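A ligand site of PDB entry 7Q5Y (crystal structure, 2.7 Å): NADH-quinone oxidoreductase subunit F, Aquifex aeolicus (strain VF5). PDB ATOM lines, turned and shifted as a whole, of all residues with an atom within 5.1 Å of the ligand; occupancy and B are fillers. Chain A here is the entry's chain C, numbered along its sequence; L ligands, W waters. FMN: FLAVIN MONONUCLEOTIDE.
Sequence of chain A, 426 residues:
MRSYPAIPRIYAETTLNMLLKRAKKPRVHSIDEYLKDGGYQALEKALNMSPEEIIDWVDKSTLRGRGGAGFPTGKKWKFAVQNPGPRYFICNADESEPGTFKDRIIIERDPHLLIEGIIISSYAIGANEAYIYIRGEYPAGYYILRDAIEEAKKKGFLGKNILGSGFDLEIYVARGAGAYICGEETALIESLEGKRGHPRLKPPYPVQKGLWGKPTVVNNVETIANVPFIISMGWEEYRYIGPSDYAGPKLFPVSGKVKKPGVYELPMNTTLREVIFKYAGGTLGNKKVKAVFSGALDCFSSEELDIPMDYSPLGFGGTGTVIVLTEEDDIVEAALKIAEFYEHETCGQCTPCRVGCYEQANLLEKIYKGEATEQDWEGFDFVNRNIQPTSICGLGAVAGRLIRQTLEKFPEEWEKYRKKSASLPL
The backbone carbonyl oxygen of Gly 183 lies close to a nitrogen (N10) of the ligand. An oxygen (O5') of the ligand sits close to the backbone carbonyl oxygen (O) of Val 218 (3.3 Å). Merely in contact with the ligand: Gly 65 (3.4 Å), Arg 66 (3.6 Å), Ala 69 (3.96 Å), Asp 94 (3.9 Å), Ser 96 (3.8 Å), Tyr 180 (3.4 Å), Glu 184 (3.6 Å), Gly 394 (3.7 Å) and Leu 395 (3.8 Å). Hydrophobic or aromatic side chains that line the ligand: Ala 69, Tyr 180, Val 218 and Leu 395.
The side-chain carboxylate of Asp 103 sits at hydrogen-bond distance from the side-chain amide nitrogen of Asn 220. The side-chain hydroxyl of Thr 223 sits at hydrogen-bond distance from the backbone NH of Arg 66. The side-chain amino group (NZ) of Lys 76 lies within salt-bridge range of the side-chain carboxylate (OE1) of Glu 185 (3.9 Å). The backbone carbonyl oxygen (O) of Val 218 sits at hydrogen-bond distance from the side-chain amino group (NZ) of Lys 76 (3.0 Å). OD1 of Asn 92 lies within hydrogen-bond range of N of Asp 94 (3.1 Å). The backbone carbonyl oxygen (O) of Asn 92 sits close to the backbone NH (N) of Val 221, 3.5 Å away. The backbone NH (N) of Gly 65 sits at hydrogen-bond distance from the backbone carbonyl oxygen (O) of Phe 71 (2.9 Å). O of Asp 94 is in hydrogen-bond range of OG of Ser 96.
The backbone NH (N) of Asn 220 lies within hydrogen-bond range of an oxygen (O3P) of the ligand (3.0 Å). The side-chain amide nitrogen (ND2) of Asn 220 lies within hydrogen-bond range of an oxygen (O2) of the ligand (2.6 Å). O3P of the ligand lies within hydrogen-bond range of OG1 of Thr 223, at 2.6 Å. NZ of Lys 76 is in salt-bridge range of O2P of the ligand, 2.7 Å away. The backbone NH (N) of Gly 67 is in hydrogen-bond range of an oxygen (O1P) of the ligand (2.8 Å). An oxygen (O3P) of the ligand lies within hydrogen-bond range of the side-chain amide nitrogen (ND2) of Asn 219, at 3.0 Å. An oxygen (O4) of the ligand is in hydrogen-bond range of the backbone NH of Glu 95, 3.1 Å away. The side-chain amide nitrogen (ND2) of Asn 92 is in hydrogen-bond range of an oxygen (O4') of the ligand, at 3.2 Å. The backbone NH of Glu 185 sits at hydrogen-bond distance from an oxygen (O2') of the ligand.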
ATOM      1  N   GLY A  65      13.191 -26.739 -23.277  1.00  0.00           N
ATOM      2  CA  GLY A  65      13.512 -25.385 -22.889  1.00  0.00           C
ATOM      3  C   GLY A  65      12.348 -24.418 -22.997  1.00  0.00           C
ATOM      4  O   GLY A  65      11.670 -24.366 -24.032  1.00  0.00           O
ATOM      5  N   ARG A  66      12.120 -23.658 -21.944  1.00  0.00           N
ATOM      6  CA  ARG A  66      11.049 -22.677 -21.878  1.00  0.00           C
ATOM      7  C   ARG A  66      11.468 -21.313 -22.435  1.00  0.00           C
ATOM      8  O   ARG A  66      10.676 -20.354 -22.376  1.00  0.00           O
ATOM      9  CB  ARG A  66      10.581 -22.528 -20.427  1.00  0.00           C
ATOM     10  CG  ARG A  66      10.290 -23.823 -19.711  1.00  0.00           C
ATOM     11  CD  ARG A  66       9.083 -24.507 -20.295  1.00  0.00           C
ATOM     12  NE  ARG A  66       8.510 -25.557 -19.449  1.00  0.00           N
ATOM     13  CZ  ARG A  66       8.510 -26.849 -19.770  1.00  0.00           C
ATOM     14  NH1 ARG A  66       7.946 -27.752 -18.967  1.00  0.00           N
ATOM     15  NH2 ARG A  66       9.084 -27.257 -20.896  1.00  0.00           N
ATOM     16  N   GLY A  67      12.696 -21.191 -22.963  1.00  0.00           N
ATOM     17  CA  GLY A  67      13.193 -19.931 -23.474  1.00  0.00           C
ATOM     18  C   GLY A  67      12.655 -19.471 -24.822  1.00  0.00           C
ATOM     19  O   GLY A  67      12.893 -18.321 -25.189  1.00  0.00           O
ATOM     20  N   GLY A  68      11.919 -20.312 -25.548  1.00  0.00           N
ATOM     21  CA  GLY A  68      11.362 -19.949 -26.840  1.00  0.00           C
ATOM     22  C   GLY A  68      11.727 -20.899 -27.978  1.00  0.00           C
ATOM     23  O   GLY A  68      10.979 -20.993 -28.952  1.00  0.00           O
ATOM     24  N   ALA A  69      12.858 -21.589 -27.871  1.00  0.00           N
ATOM     25  CA  ALA A  69      13.301 -22.520 -28.906  1.00  0.00           C
ATOM     26  C   ALA A  69      12.849 -23.963 -28.692  1.00  0.00           C
ATOM     27  O   ALA A  69      12.999 -24.796 -29.593  1.00  0.00           O
ATOM     28  CB  ALA A  69      14.826 -22.480 -29.033  1.00  0.00           C
ATOM     29  N   GLY A  70      12.310 -24.292 -27.525  1.00  0.00           N
ATOM     30  CA  GLY A  70      11.866 -25.630 -27.225  1.00  0.00           C
ATOM     31  C   GLY A  70      12.876 -26.757 -27.411  1.00  0.00           C
ATOM     32  O   GLY A  70      12.472 -27.888 -27.669  1.00  0.00           O
ATOM     33  N   PHE A  71      14.177 -26.482 -27.264  1.00  0.00           N
ATOM     34  CA  PHE A  71      15.123 -27.585 -27.438  1.00  0.00           C
ATOM     35  C   PHE A  71      15.162 -28.486 -26.187  1.00  0.00           C
ATOM     36  O   PHE A  71      15.094 -27.989 -25.065  1.00  0.00           O
ATOM     37  CB  PHE A  71      16.515 -27.036 -27.719  1.00  0.00           C
ATOM     38  CG  PHE A  71      17.443 -28.064 -28.268  1.00  0.00           C
ATOM     39  CD1 PHE A  71      18.248 -28.811 -27.412  1.00  0.00           C
ATOM     40  CD2 PHE A  71      17.464 -28.329 -29.624  1.00  0.00           C
ATOM     41  CE1 PHE A  71      19.088 -29.782 -27.913  1.00  0.00           C
ATOM     42  CE2 PHE A  71      18.312 -29.296 -30.130  1.00  0.00           C
ATOM     43  CZ  PHE A  71      19.119 -30.021 -29.269  1.00  0.00           C
ATOM     44  N   LYS A  76      20.641 -31.040 -24.748  1.00  0.00           N
ATOM     45  CA  LYS A  76      21.588 -29.939 -24.760  1.00  0.00           C
ATOM     46  C   LYS A  76      22.719 -30.231 -23.777  1.00  0.00           C
ATOM     47  O   LYS A  76      23.900 -30.034 -24.089  1.00  0.00           O
ATOM     48  CB  LYS A  76      20.876 -28.612 -24.449  1.00  0.00           C
ATOM     49  CG  LYS A  76      21.791 -27.380 -24.253  1.00  0.00           C
ATOM     50  CD  LYS A  76      20.987 -26.180 -23.723  1.00  0.00           C
ATOM     51  CE  LYS A  76      20.125 -25.606 -24.814  1.00  0.00           C
ATOM     52  NZ  LYS A  76      19.430 -24.381 -24.382  1.00  0.00           N
ATOM     53  N   ASN A  92      19.786 -17.803 -18.027  1.00  0.00           N
ATOM     54  CA  ASN A  92      19.326 -16.687 -18.846  1.00  0.00           C
ATOM     55  C   ASN A  92      18.097 -16.013 -18.241  1.00  0.00           C
ATOM     56  O   ASN A  92      16.974 -16.491 -18.373  1.00  0.00           O
ATOM     57  CB  ASN A  92      19.021 -17.171 -20.247  1.00  0.00           C
ATOM     58  CG  ASN A  92      18.820 -16.057 -21.178  1.00  0.00           C
ATOM     59  OD1 ASN A  92      18.499 -14.935 -20.759  1.00  0.00           O
ATOM     60  ND2 ASN A  92      18.986 -16.329 -22.462  1.00  0.00           N
ATOM     61  N   ASP A  94      17.319 -12.703 -18.994  1.00  0.00           N
ATOM     62  CA  ASP A  94      17.206 -11.428 -19.680  1.00  0.00           C
ATOM     63  C   ASP A  94      15.744 -10.991 -19.795  1.00  0.00           C
ATOM     64  O   ASP A  94      15.438  -9.813 -19.588  1.00  0.00           O
ATOM     65  CB  ASP A  94      17.917 -11.478 -21.018  1.00  0.00           C
ATOM     66  CG  ASP A  94      17.976 -10.138 -21.662  1.00  0.00           C
ATOM     67  OD1 ASP A  94      18.754  -9.294 -21.164  1.00  0.00           O
ATOM     68  OD2 ASP A  94      17.232  -9.947 -22.657  1.00  0.00           O
ATOM     69  N   GLU A  95      14.828 -11.900 -20.137  1.00  0.00           N
ATOM     70  CA  GLU A  95      13.385 -11.659 -20.195  1.00  0.00           C
ATOM     71  C   GLU A  95      12.974 -10.258 -20.631  1.00  0.00           C
ATOM     72  O   GLU A  95      12.634  -9.422 -19.774  1.00  0.00           O
ATOM     73  CB  GLU A  95      12.701 -11.975 -18.867  1.00  0.00           C
ATOM     74  CG  GLU A  95      11.169 -11.914 -19.017  1.00  0.00           C
ATOM     75  CD  GLU A  95      10.388 -12.576 -17.887  1.00  0.00           C
ATOM     76  OE1 GLU A  95      10.403 -12.028 -16.757  1.00  0.00           O
ATOM     77  OE2 GLU A  95       9.758 -13.645 -18.162  1.00  0.00           O
ATOM     78  N   SER A  96      13.116  -9.939 -21.903  1.00  0.00           N
ATOM     79  CA  SER A  96      12.747  -8.600 -22.358  1.00  0.00           C
ATOM     80  C   SER A  96      11.728  -8.595 -23.493  1.00  0.00           C
ATOM     81  O   SER A  96      11.513  -7.545 -24.100  1.00  0.00           O
ATOM     82  CB  SER A  96      14.004  -7.844 -22.766  1.00  0.00           C
ATOM     83  OG  SER A  96      14.842  -7.713 -21.636  1.00  0.00           O
ATOM     84  N   ASP A 103       9.369 -15.009 -15.756  1.00  0.00           N
ATOM     85  CA  ASP A 103      10.608 -15.288 -15.033  1.00  0.00           C
ATOM     86  C   ASP A 103      10.790 -14.384 -13.813  1.00  0.00           C
ATOM     87  O   ASP A 103      11.319 -14.826 -12.782  1.00  0.00           O
ATOM     88  CB  ASP A 103      11.792 -15.197 -15.992  1.00  0.00           C
ATOM     89  CG  ASP A 103      11.621 -16.098 -17.251  1.00  0.00           C
ATOM     90  OD1 ASP A 103      10.916 -17.138 -17.182  1.00  0.00           O
ATOM     91  OD2 ASP A 103      12.194 -15.786 -18.313  1.00  0.00           O
ATOM     92  N   TYR A 180      17.315  -6.152 -25.718  1.00  0.00           N
ATOM     93  CA  TYR A 180      16.535  -7.379 -25.785  1.00  0.00           C
ATOM     94  C   TYR A 180      17.340  -8.477 -26.469  1.00  0.00           C
ATOM     95  O   TYR A 180      17.172  -9.662 -26.154  1.00  0.00           O
ATOM     96  CB  TYR A 180      15.218  -7.102 -26.518  1.00  0.00           C
ATOM     97  CG  TYR A 180      14.496  -8.293 -27.106  1.00  0.00           C
ATOM     98  CD1 TYR A 180      13.693  -9.137 -26.322  1.00  0.00           C
ATOM     99  CD2 TYR A 180      14.603  -8.599 -28.459  1.00  0.00           C
ATOM    100  CE1 TYR A 180      13.029 -10.229 -26.874  1.00  0.00           C
ATOM    101  CE2 TYR A 180      13.934  -9.674 -29.001  1.00  0.00           C
ATOM    102  CZ  TYR A 180      13.155 -10.488 -28.217  1.00  0.00           C
ATOM    103  OH  TYR A 180      12.511 -11.543 -28.804  1.00  0.00           O
ATOM    104  N   ILE A 181      18.241  -8.090 -27.364  1.00  0.00           N
ATOM    105  CA  ILE A 181      19.069  -9.046 -28.078  1.00  0.00           C
ATOM    106  C   ILE A 181      19.971  -9.834 -27.130  1.00  0.00           C
ATOM    107  O   ILE A 181      20.361 -10.964 -27.445  1.00  0.00           O
ATOM    108  CB  ILE A 181      19.867  -8.291 -29.177  1.00  0.00           C
ATOM    109  CG1 ILE A 181      20.612  -9.258 -30.088  1.00  0.00           C
ATOM    110  CG2 ILE A 181      20.839  -7.284 -28.595  1.00  0.00           C
ATOM    111  CD1 ILE A 181      19.731 -10.306 -30.643  1.00  0.00           C
ATOM    112  N   GLY A 183      19.225 -11.497 -24.825  1.00  0.00           N
ATOM    113  CA  GLY A 183      18.565 -12.721 -24.444  1.00  0.00           C
ATOM    114  C   GLY A 183      18.929 -13.833 -25.407  1.00  0.00           C
ATOM    115  O   GLY A 183      18.670 -15.007 -25.129  1.00  0.00           O
ATOM    116  N   GLU A 184      19.502 -13.463 -26.549  1.00  0.00           N
ATOM    117  CA  GLU A 184      19.960 -14.436 -27.527  1.00  0.00           C
ATOM    118  C   GLU A 184      21.217 -15.096 -26.956  1.00  0.00           C
ATOM    119  O   GLU A 184      22.145 -14.394 -26.539  1.00  0.00           O
ATOM    120  CB  GLU A 184      20.283 -13.742 -28.860  1.00  0.00           C
ATOM    121  CG  GLU A 184      20.263 -14.601 -30.108  1.00  0.00           C
ATOM    122  CD  GLU A 184      21.567 -15.334 -30.360  1.00  0.00           C
ATOM    123  OE1 GLU A 184      22.536 -15.154 -29.602  1.00  0.00           O
ATOM    124  OE2 GLU A 184      21.623 -16.110 -31.336  1.00  0.00           O
ATOM    125  N   GLU A 185      21.235 -16.433 -26.949  1.00  0.00           N
ATOM    126  CA  GLU A 185      22.322 -17.255 -26.412  1.00  0.00           C
ATOM    127  C   GLU A 185      23.741 -16.724 -26.653  1.00  0.00           C
ATOM    128  O   GLU A 185      24.511 -16.525 -25.707  1.00  0.00           O
ATOM    129  CB  GLU A 185      22.170 -18.648 -27.009  1.00  0.00           C
ATOM    130  CG  GLU A 185      22.585 -19.800 -26.187  1.00  0.00           C
ATOM    131  CD  GLU A 185      22.347 -21.080 -26.949  1.00  0.00           C
ATOM    132  OE1 GLU A 185      21.581 -21.936 -26.451  1.00  0.00           O
ATOM    133  OE2 GLU A 185      22.909 -21.212 -28.067  1.00  0.00           O
ATOM    134  N   VAL A 218      23.347 -22.658 -21.749  1.00  0.00           N
ATOM    135  CA  VAL A 218      22.487 -21.524 -21.432  1.00  0.00           C
ATOM    136  C   VAL A 218      21.077 -22.054 -21.272  1.00  0.00           C
ATOM    137  O   VAL A 218      20.553 -22.707 -22.170  1.00  0.00           O
ATOM    138  CB  VAL A 218      22.490 -20.438 -22.515  1.00  0.00           C
ATOM    139  CG1 VAL A 218      21.449 -19.355 -22.125  1.00  0.00           C
ATOM    140  CG2 VAL A 218      23.900 -19.818 -22.688  1.00  0.00           C
ATOM    141  N   ASN A 219      20.449 -21.761 -20.133  1.00  0.00           N
ATOM    142  CA  ASN A 219      19.089 -22.232 -19.929  1.00  0.00           C
ATOM    143  C   ASN A 219      18.244 -21.114 -19.358  1.00  0.00           C
ATOM    144  O   ASN A 219      18.723 -20.287 -18.572  1.00  0.00           O
ATOM    145  CB  ASN A 219      19.031 -23.475 -19.006  1.00  0.00           C
ATOM    146  CG  ASN A 219      19.168 -24.785 -19.786  1.00  0.00           C
ATOM    147  OD1 ASN A 219      19.976 -25.657 -19.440  1.00  0.00           O
ATOM    148  ND2 ASN A 219      18.387 -24.921 -20.843  1.00  0.00           N
ATOM    149  N   ASN A 220      16.982 -21.100 -19.760  1.00  0.00           N
ATOM    150  CA  ASN A 220      16.041 -20.113 -19.286  1.00  0.00           C
ATOM    151  C   ASN A 220      15.703 -20.391 -17.821  1.00  0.00           C
ATOM    152  O   ASN A 220      15.747 -21.532 -17.353  1.00  0.00           O
ATOM    153  CB  ASN A 220      14.775 -20.130 -20.142  1.00  0.00           C
ATOM    154  CG  ASN A 220      13.663 -19.251 -19.595  1.00  0.00           C
ATOM    155  OD1 ASN A 220      12.690 -19.741 -19.040  1.00  0.00           O
ATOM    156  ND2 ASN A 220      13.828 -17.948 -19.749  1.00  0.00           N
ATOM    157  N   VAL A 221      15.359 -19.308 -17.105  1.00  0.00           N
ATOM    158  CA  VAL A 221      14.999 -19.382 -15.693  1.00  0.00           C
ATOM    159  C   VAL A 221      13.882 -20.399 -15.471  1.00  0.00           C
ATOM    160  O   VAL A 221      13.960 -21.240 -14.570  1.00  0.00           O
ATOM    161  CB  VAL A 221      14.610 -17.976 -15.182  1.00  0.00           C
ATOM    162  CG1 VAL A 221      14.028 -18.043 -13.794  1.00  0.00           C
ATOM    163  CG2 VAL A 221      15.810 -17.033 -15.266  1.00  0.00           C
ATOM    164  N   THR A 223      13.070 -22.976 -17.307  1.00  0.00           N
ATOM    165  CA  THR A 223      13.586 -24.318 -17.532  1.00  0.00           C
ATOM    166  C   THR A 223      14.297 -24.831 -16.285  1.00  0.00           C
ATOM    167  O   THR A 223      14.061 -25.964 -15.843  1.00  0.00           O
ATOM    168  CB  THR A 223      14.572 -24.346 -18.713  1.00  0.00           C
ATOM    169  OG1 THR A 223      13.996 -23.723 -19.851  1.00  0.00           O
ATOM    170  CG2 THR A 223      14.900 -25.756 -19.080  1.00  0.00           C
ATOM    171  N   CYS A 393      20.589 -13.845 -36.812  1.00  0.00           N
ATOM    172  CA  CYS A 393      19.968 -14.424 -35.638  1.00  0.00           C
ATOM    173  C   CYS A 393      18.428 -14.402 -35.663  1.00  0.00           C
ATOM    174  O   CYS A 393      17.768 -13.901 -36.587  1.00  0.00           O
ATOM    175  CB  CYS A 393      20.498 -13.712 -34.393  1.00  0.00           C
ATOM    176  SG  CYS A 393      19.619 -12.190 -33.937  1.00  0.00           S
ATOM    177  N   GLY A 394      17.856 -14.978 -34.594  1.00  0.00           N
ATOM    178  CA  GLY A 394      16.409 -15.094 -34.468  1.00  0.00           C
ATOM    179  C   GLY A 394      15.657 -13.781 -34.471  1.00  0.00           C
ATOM    180  O   GLY A 394      14.509 -13.735 -34.902  1.00  0.00           O
ATOM    181  N   LEU A 395      16.275 -12.704 -33.994  1.00  0.00           N
ATOM    182  CA  LEU A 395      15.574 -11.425 -33.999  1.00  0.00           C
ATOM    183  C   LEU A 395      15.177 -11.020 -35.419  1.00  0.00           C
ATOM    184  O   LEU A 395      14.011 -10.797 -35.712  1.00  0.00           O
ATOM    185  CB  LEU A 395      16.421 -10.340 -33.340  1.00  0.00           C
ATOM    186  CG  LEU A 395      15.661  -9.062 -32.985  1.00  0.00           C
ATOM    187  CD1 LEU A 395      16.384  -8.349 -31.843  1.00  0.00           C
ATOM    188  CD2 LEU A 395      15.513  -8.110 -34.184  1.00  0.00           C
HETATM  189  N1  FMN L   1      15.827 -16.996 -23.838  1.00  0.00           N
HETATM  190  C2  FMN L   1      15.503 -16.655 -22.534  1.00  0.00           C
HETATM  191  O2  FMN L   1      15.530 -17.523 -21.650  1.00  0.00           O
HETATM  192  N3  FMN L   1      15.174 -15.336 -22.212  1.00  0.00           N
HETATM  193  C4  FMN L   1      15.153 -14.352 -23.192  1.00  0.00           C
HETATM  194  O4  FMN L   1      14.875 -13.160 -22.935  1.00  0.00           O
HETATM  195  C4A FMN L   1      15.460 -14.724 -24.490  1.00  0.00           C
HETATM  196  N5  FMN L   1      15.438 -13.754 -25.445  1.00  0.00           N
HETATM  197  C5A FMN L   1      15.759 -14.041 -26.742  1.00  0.00           C
HETATM  198  C6  FMN L   1      15.728 -12.998 -27.663  1.00  0.00           C
HETATM  199  C7  FMN L   1      16.025 -13.254 -28.983  1.00  0.00           C
HETATM  200  C7M FMN L   1      16.006 -12.135 -29.989  1.00  0.00           C
HETATM  201  C8  FMN L   1      16.352 -14.551 -29.382  1.00  0.00           C
HETATM  202  C8M FMN L   1      16.694 -14.772 -30.822  1.00  0.00           C
HETATM  203  C9  FMN L   1      16.383 -15.593 -28.462  1.00  0.00           C
HETATM  204  C9A FMN L   1      16.084 -15.344 -27.112  1.00  0.00           C
HETATM  205  N10 FMN L   1      16.093 -16.346 -26.127  1.00  0.00           N
HETATM  206  C10 FMN L   1      15.787 -16.027 -24.819  1.00  0.00           C
HETATM  207  C1' FMN L   1      16.417 -17.768 -26.437  1.00  0.00           C
HETATM  208  C2' FMN L   1      17.866 -18.114 -26.219  1.00  0.00           C
HETATM  209  O2' FMN L   1      18.441 -17.891 -27.472  1.00  0.00           O
HETATM  210  C3' FMN L   1      18.023 -19.604 -25.897  1.00  0.00           C
HETATM  211  O3' FMN L   1      17.470 -20.408 -26.934  1.00  0.00           O
HETATM  212  C4' FMN L   1      17.449 -20.006 -24.519  1.00  0.00           C
HETATM  213  O4' FMN L   1      17.742 -19.036 -23.529  1.00  0.00           O
HETATM  214  C5' FMN L   1      17.978 -21.384 -24.133  1.00  0.00           C
HETATM  215  O5' FMN L   1      17.416 -21.833 -22.914  1.00  0.00           O
HETATM  216  P   FMN L   1      16.279 -22.984 -22.935  1.00  0.00           P
HETATM  217  O1P FMN L   1      15.068 -22.467 -23.688  1.00  0.00           O
HETATM  218  O2P FMN L   1      16.824 -24.145 -23.718  1.00  0.00           O
HETATM  219  O3P FMN L   1      15.941 -23.316 -21.519  1.00  0.00           O
HETATM  220  O   HOH W   1      14.706 -14.908 -19.421  1.00  0.00           O
